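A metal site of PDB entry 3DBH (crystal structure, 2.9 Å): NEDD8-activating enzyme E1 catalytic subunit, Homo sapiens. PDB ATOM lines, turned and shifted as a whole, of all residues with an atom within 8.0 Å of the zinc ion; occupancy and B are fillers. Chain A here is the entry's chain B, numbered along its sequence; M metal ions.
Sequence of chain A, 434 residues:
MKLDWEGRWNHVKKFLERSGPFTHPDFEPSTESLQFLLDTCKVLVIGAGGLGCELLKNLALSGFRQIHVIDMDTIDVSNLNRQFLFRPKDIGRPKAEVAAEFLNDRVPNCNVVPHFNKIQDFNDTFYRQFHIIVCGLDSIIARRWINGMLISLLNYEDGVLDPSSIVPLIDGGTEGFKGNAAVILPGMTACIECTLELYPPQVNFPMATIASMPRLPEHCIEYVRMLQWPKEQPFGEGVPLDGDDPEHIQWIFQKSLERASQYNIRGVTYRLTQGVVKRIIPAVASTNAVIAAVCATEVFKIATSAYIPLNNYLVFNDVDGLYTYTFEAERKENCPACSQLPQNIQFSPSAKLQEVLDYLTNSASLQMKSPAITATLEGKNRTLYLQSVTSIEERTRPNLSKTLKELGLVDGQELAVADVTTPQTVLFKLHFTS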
ATOM      1  N   ASN A 147      26.870  14.408  13.836  1.00  0.00           N
ATOM      2  CA  ASN A 147      27.567  13.742  14.918  1.00  0.00           C
ATOM      3  C   ASN A 147      28.425  12.643  14.284  1.00  0.00           C
ATOM      4  O   ASN A 147      29.636  12.595  14.497  1.00  0.00           O
ATOM      5  CB  ASN A 147      26.529  13.145  15.887  1.00  0.00           C
ATOM      6  CG  ASN A 147      27.156  12.479  17.089  1.00  0.00           C
ATOM      7  OD1 ASN A 147      27.807  13.125  17.899  1.00  0.00           O
ATOM      8  ND2 ASN A 147      26.943  11.185  17.210  1.00  0.00           N
ATOM      9  N   ILE A 151      32.644  11.963  14.290  1.00  0.00           N
ATOM     10  CA  ILE A 151      33.248  10.814  14.964  1.00  0.00           C
ATOM     11  C   ILE A 151      34.063  10.100  13.894  1.00  0.00           C
ATOM     12  O   ILE A 151      35.051   9.434  14.191  1.00  0.00           O
ATOM     13  CB  ILE A 151      32.184   9.875  15.528  1.00  0.00           C
ATOM     14  CG1 ILE A 151      31.500  10.534  16.700  1.00  0.00           C
ATOM     15  CG2 ILE A 151      32.816   8.617  16.012  1.00  0.00           C
ATOM     16  CD1 ILE A 151      30.273   9.787  17.176  1.00  0.00           C
ATOM     17  N   ILE A 184      30.198  18.618  22.703  1.00  0.00           N
ATOM     18  CA  ILE A 184      30.604  17.263  22.392  1.00  0.00           C
ATOM     19  C   ILE A 184      32.042  17.182  21.861  1.00  0.00           C
ATOM     20  O   ILE A 184      32.388  17.834  20.880  1.00  0.00           O
ATOM     21  CB  ILE A 184      29.636  16.648  21.356  1.00  0.00           C
ATOM     22  CG1 ILE A 184      28.205  16.700  21.889  1.00  0.00           C
ATOM     23  CG2 ILE A 184      30.062  15.226  21.035  1.00  0.00           C
ATOM     24  CD1 ILE A 184      27.189  15.951  21.045  1.00  0.00           C
ATOM     25  N   PRO A 186      34.011  14.563  20.271  1.00  0.00           N
ATOM     26  CA  PRO A 186      34.019  13.217  19.690  1.00  0.00           C
ATOM     27  C   PRO A 186      35.189  12.416  20.227  1.00  0.00           C
ATOM     28  O   PRO A 186      36.312  12.914  20.286  1.00  0.00           O
ATOM     29  CB  PRO A 186      34.129  13.489  18.196  1.00  0.00           C
ATOM     30  CG  PRO A 186      33.392  14.773  18.043  1.00  0.00           C
ATOM     31  CD  PRO A 186      33.907  15.585  19.220  1.00  0.00           C
ATOM     32  N   GLY A 187      34.933  11.193  20.659  1.00  0.00           N
ATOM     33  CA  GLY A 187      36.013  10.379  21.178  1.00  0.00           C
ATOM     34  C   GLY A 187      36.043  10.329  22.689  1.00  0.00           C
ATOM     35  O   GLY A 187      36.176   9.253  23.271  1.00  0.00           O
ATOM     36  N   MET A 188      35.916  11.494  23.325  1.00  0.00           N
ATOM     37  CA  MET A 188      35.915  11.597  24.776  1.00  0.00           C
ATOM     38  C   MET A 188      34.501  11.809  25.315  1.00  0.00           C
ATOM     39  O   MET A 188      33.824  10.838  25.662  1.00  0.00           O
ATOM     40  CB  MET A 188      36.859  12.713  25.170  1.00  0.00           C
ATOM     41  CG  MET A 188      38.291  12.341  24.804  1.00  0.00           C
ATOM     42  SD  MET A 188      39.472  13.707  24.808  1.00  0.00           S
ATOM     43  CE  MET A 188      39.424  14.264  26.600  1.00  0.00           C
ATOM     44  N   THR A 189      34.052  13.055  25.394  1.00  0.00           N
ATOM     45  CA  THR A 189      32.703  13.412  25.855  1.00  0.00           C
ATOM     46  C   THR A 189      31.552  12.591  25.216  1.00  0.00           C
ATOM     47  O   THR A 189      31.710  12.034  24.128  1.00  0.00           O
ATOM     48  CB  THR A 189      32.450  14.911  25.578  1.00  0.00           C
ATOM     49  OG1 THR A 189      32.960  15.685  26.673  1.00  0.00           O
ATOM     50  CG2 THR A 189      30.964  15.222  25.372  1.00  0.00           C
ATOM     51  N   ALA A 190      30.405  12.537  25.892  1.00  0.00           N
ATOM     52  CA  ALA A 190      29.229  11.831  25.371  1.00  0.00           C
ATOM     53  C   ALA A 190      28.792  12.485  24.066  1.00  0.00           C
ATOM     54  O   ALA A 190      28.811  13.712  23.973  1.00  0.00           O
ATOM     55  CB  ALA A 190      28.095  11.904  26.374  1.00  0.00           C
ATOM     56  N   CYS A 191      28.395  11.694  23.076  1.00  0.00           N
ATOM     57  CA  CYS A 191      27.973  12.261  21.804  1.00  0.00           C
ATOM     58  C   CYS A 191      26.437  12.349  21.693  1.00  0.00           C
ATOM     59  O   CYS A 191      25.728  12.008  22.649  1.00  0.00           O
ATOM     60  CB  CYS A 191      28.534  11.427  20.643  1.00  0.00           C
ATOM     61  SG  CYS A 191      27.664   9.876  20.239  1.00  0.00           S
ATOM     62  N   ILE A 192      25.926  12.842  20.566  1.00  0.00           N
ATOM     63  CA  ILE A 192      24.480  12.965  20.340  1.00  0.00           C
ATOM     64  C   ILE A 192      23.809  11.613  20.505  1.00  0.00           C
ATOM     65  O   ILE A 192      22.763  11.480  21.164  1.00  0.00           O
ATOM     66  CB  ILE A 192      24.160  13.465  18.898  1.00  0.00           C
ATOM     67  CG1 ILE A 192      24.636  14.912  18.718  1.00  0.00           C
ATOM     68  CG2 ILE A 192      22.663  13.345  18.621  1.00  0.00           C
ATOM     69  CD1 ILE A 192      23.852  15.936  19.511  1.00  0.00           C
ATOM     70  N   GLU A 193      24.404  10.596  19.894  1.00  0.00           N
ATOM     71  CA  GLU A 193      23.875   9.262  19.965  1.00  0.00           C
ATOM     72  C   GLU A 193      23.844   8.770  21.414  1.00  0.00           C
ATOM     73  O   GLU A 193      22.928   8.052  21.806  1.00  0.00           O
ATOM     74  CB  GLU A 193      24.722   8.322  19.109  1.00  0.00           C
ATOM     75  CG  GLU A 193      23.900   7.355  18.295  1.00  0.00           C
ATOM     76  CD  GLU A 193      23.114   8.039  17.188  1.00  0.00           C
ATOM     77  OE1 GLU A 193      21.940   7.653  16.984  1.00  0.00           O
ATOM     78  OE2 GLU A 193      23.668   8.937  16.507  1.00  0.00           O
ATOM     79  N   CYS A 194      24.855   9.163  22.204  1.00  0.00           N
ATOM     80  CA  CYS A 194      24.953   8.793  23.615  1.00  0.00           C
ATOM     81  C   CYS A 194      23.717   9.258  24.364  1.00  0.00           C
ATOM     82  O   CYS A 194      23.068   8.494  25.093  1.00  0.00           O
ATOM     83  CB  CYS A 194      26.163   9.454  24.277  1.00  0.00           C
ATOM     84  SG  CYS A 194      27.743   8.653  24.032  1.00  0.00           S
ATOM     85  N   THR A 195      23.378  10.525  24.180  1.00  0.00           N
ATOM     86  CA  THR A 195      22.232  11.110  24.844  1.00  0.00           C
ATOM     87  C   THR A 195      20.998  11.171  23.958  1.00  0.00           C
ATOM     88  O   THR A 195      20.112  11.979  24.202  1.00  0.00           O
ATOM     89  CB  THR A 195      22.584  12.531  25.363  1.00  0.00           C
ATOM     90  OG1 THR A 195      22.800  13.422  24.266  1.00  0.00           O
ATOM     91  CG2 THR A 195      23.865  12.488  26.196  1.00  0.00           C
ATOM     92  N   LEU A 196      20.930  10.295  22.954  1.00  0.00           N
ATOM     93  CA  LEU A 196      19.799  10.266  22.030  1.00  0.00           C
ATOM     94  C   LEU A 196      18.442  10.201  22.707  1.00  0.00           C
ATOM     95  O   LEU A 196      17.513  10.851  22.265  1.00  0.00           O
ATOM     96  CB  LEU A 196      19.893   9.071  21.069  1.00  0.00           C
ATOM     97  CG  LEU A 196      18.818   8.993  19.962  1.00  0.00           C
ATOM     98  CD1 LEU A 196      18.927  10.221  19.065  1.00  0.00           C
ATOM     99  CD2 LEU A 196      19.004   7.735  19.115  1.00  0.00           C
ATOM    100  N   GLU A 330      27.174  11.125  31.126  1.00  0.00           N
ATOM    101  CA  GLU A 330      28.107  10.013  30.952  1.00  0.00           C
ATOM    102  C   GLU A 330      28.136   9.545  29.500  1.00  0.00           C
ATOM    103  O   GLU A 330      27.123   9.529  28.820  1.00  0.00           O
ATOM    104  CB  GLU A 330      27.707   8.814  31.828  1.00  0.00           C
ATOM    105  CG  GLU A 330      27.507   9.118  33.314  1.00  0.00           C
ATOM    106  CD  GLU A 330      28.804   9.425  34.058  1.00  0.00           C
ATOM    107  OE1 GLU A 330      29.622   8.491  34.212  1.00  0.00           O
ATOM    108  OE2 GLU A 330      28.982  10.590  34.491  1.00  0.00           O
ATOM    109  N   ARG A 331      29.312   9.155  29.035  1.00  0.00           N
ATOM    110  CA  ARG A 331      29.441   8.667  27.683  1.00  0.00           C
ATOM    111  C   ARG A 331      29.038   7.202  27.642  1.00  0.00           C
ATOM    112  O   ARG A 331      29.830   6.359  28.024  1.00  0.00           O
ATOM    113  CB  ARG A 331      30.878   8.816  27.211  1.00  0.00           C
ATOM    114  CG  ARG A 331      31.147   8.087  25.912  1.00  0.00           C
ATOM    115  CD  ARG A 331      32.623   7.968  25.610  1.00  0.00           C
ATOM    116  NE  ARG A 331      32.839   7.240  24.362  1.00  0.00           N
ATOM    117  CZ  ARG A 331      34.034   6.956  23.867  1.00  0.00           C
ATOM    118  NH1 ARG A 331      35.128   7.330  24.511  1.00  0.00           N
ATOM    119  NH2 ARG A 331      34.144   6.310  22.707  1.00  0.00           N
ATOM    120  N   LYS A 332      27.827   6.905  27.186  1.00  0.00           N
ATOM    121  CA  LYS A 332      27.346   5.521  27.101  1.00  0.00           C
ATOM    122  C   LYS A 332      28.423   4.622  26.469  1.00  0.00           C
ATOM    123  O   LYS A 332      28.673   4.699  25.262  1.00  0.00           O
ATOM    124  CB  LYS A 332      26.031   5.506  26.310  1.00  0.00           C
ATOM    125  CG  LYS A 332      25.405   4.135  26.164  1.00  0.00           C
ATOM    126  CD  LYS A 332      23.920   4.209  25.796  1.00  0.00           C
ATOM    127  CE  LYS A 332      23.069   4.683  26.979  1.00  0.00           C
ATOM    128  NZ  LYS A 332      21.602   4.563  26.733  1.00  0.00           N
ATOM    129  N   GLU A 333      29.048   3.765  27.282  1.00  0.00           N
ATOM    130  CA  GLU A 333      30.162   2.890  26.879  1.00  0.00           C
ATOM    131  C   GLU A 333      29.990   1.857  25.766  1.00  0.00           C
ATOM    132  O   GLU A 333      30.975   1.393  25.191  1.00  0.00           O
ATOM    133  CB  GLU A 333      30.730   2.171  28.124  1.00  0.00           C
ATOM    134  CG  GLU A 333      31.477   3.089  29.094  1.00  0.00           C
ATOM    135  CD  GLU A 333      32.013   2.373  30.344  1.00  0.00           C
ATOM    136  OE1 GLU A 333      31.196   1.872  31.160  1.00  0.00           O
ATOM    137  OE2 GLU A 333      33.250   2.318  30.521  1.00  0.00           O
ATOM    138  N   ASN A 334      28.760   1.493  25.473  1.00  0.00           N
ATOM    139  CA  ASN A 334      28.494   0.524  24.423  1.00  0.00           C
ATOM    140  C   ASN A 334      27.784   1.245  23.279  1.00  0.00           C
ATOM    141  O   ASN A 334      26.932   0.681  22.597  1.00  0.00           O
ATOM    142  CB  ASN A 334      27.635  -0.612  24.984  1.00  0.00           C
ATOM    143  CG  ASN A 334      26.519  -0.107  25.890  1.00  0.00           C
ATOM    144  OD1 ASN A 334      25.462  -0.732  26.017  1.00  0.00           O
ATOM    145  ND2 ASN A 334      26.761   1.047  26.546  1.00  0.00           N
ATOM    146  N   CYS A 335      28.154   2.522  23.098  1.00  0.00           N
ATOM    147  CA  CYS A 335      27.554   3.371  22.064  1.00  0.00           C
ATOM    148  C   CYS A 335      27.769   2.910  20.648  1.00  0.00           C
ATOM    149  O   CYS A 335      28.844   2.458  20.251  1.00  0.00           O
ATOM    150  CB  CYS A 335      28.062   4.832  22.142  1.00  0.00           C
ATOM    151  SG  CYS A 335      27.127   6.045  21.150  1.00  0.00           S
ATOM    152  N   PRO A 336      26.726   3.044  19.851  1.00  0.00           N
ATOM    153  CA  PRO A 336      26.854   2.626  18.463  1.00  0.00           C
ATOM    154  C   PRO A 336      27.652   3.658  17.643  1.00  0.00           C
ATOM    155  O   PRO A 336      28.231   3.352  16.598  1.00  0.00           O
ATOM    156  CB  PRO A 336      25.398   2.464  18.021  1.00  0.00           C
ATOM    157  CG  PRO A 336      24.674   3.465  18.867  1.00  0.00           C
ATOM    158  CD  PRO A 336      25.310   3.275  20.213  1.00  0.00           C
ATOM    159  N   ALA A 337      27.698   4.888  18.136  1.00  0.00           N
ATOM    160  CA  ALA A 337      28.413   5.938  17.440  1.00  0.00           C
ATOM    161  C   ALA A 337      29.877   6.067  17.826  1.00  0.00           C
ATOM    162  O   ALA A 337      30.752   5.597  17.103  1.00  0.00           O
ATOM    163  CB  ALA A 337      27.708   7.285  17.663  1.00  0.00           C
ATOM    164  N   CYS A 338      30.131   6.679  18.989  1.00  0.00           N
ATOM    165  CA  CYS A 338      31.491   6.931  19.442  1.00  0.00           C
ATOM    166  C   CYS A 338      32.294   5.795  20.038  1.00  0.00           C
ATOM    167  O   CYS A 338      33.463   5.972  20.380  1.00  0.00           O
ATOM    168  CB  CYS A 338      31.489   8.107  20.412  1.00  0.00           C
ATOM    169  SG  CYS A 338      30.491   7.850  21.847  1.00  0.00           S
ATOM    170  N   SER A 339      31.675   4.630  20.195  1.00  0.00           N
ATOM    171  CA  SER A 339      32.416   3.506  20.731  1.00  0.00           C
ATOM    172  C   SER A 339      33.153   2.831  19.603  1.00  0.00           C
ATOM    173  O   SER A 339      32.839   3.020  18.441  1.00  0.00           O
ATOM    174  CB  SER A 339      31.489   2.503  21.384  1.00  0.00           C
ATOM    175  OG  SER A 339      32.228   1.343  21.684  1.00  0.00           O
HETATM  176 ZN    ZN M   1      28.280   8.117  21.816  1.00  0.00          ZN
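The guanidinium group of Arg 331 is in hydrogen-bond range of the backbone carbonyl oxygen of Cys 338 (2.4 Å). The backbone NH of Lys 332 sits close to the side-chain sulfur of Cys 194 (3.6 Å). The side-chain sulfur (SG) of Cys 191 sits close to the backbone NH (N) of Glu 193 (3.4 Å). The side-chain amide nitrogen (ND2) of Asn 147 lies close to the side-chain sulfur (SG) of Cys 191 (3.4 Å). The side-chain sulfur of Cys 335 lies close to the backbone NH of Ala 337, at 3.3 Å.
Four residues have an atom within 4 Å of the zinc ion: Cys 191, Cys 194, Cys 335 and Cys 338. The nearest printed residue that does not touch the zinc ion is Ala 337 (4.3 Å).
The zinc ion is bound by SG of Cys 338 (2.2 Å), SG of Cys 194 (2.3 Å), SG of Cys 191 (2.4 Å) and SG of Cys 335 (2.5 Å). The zinc ion has four donor atoms within binding distance.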
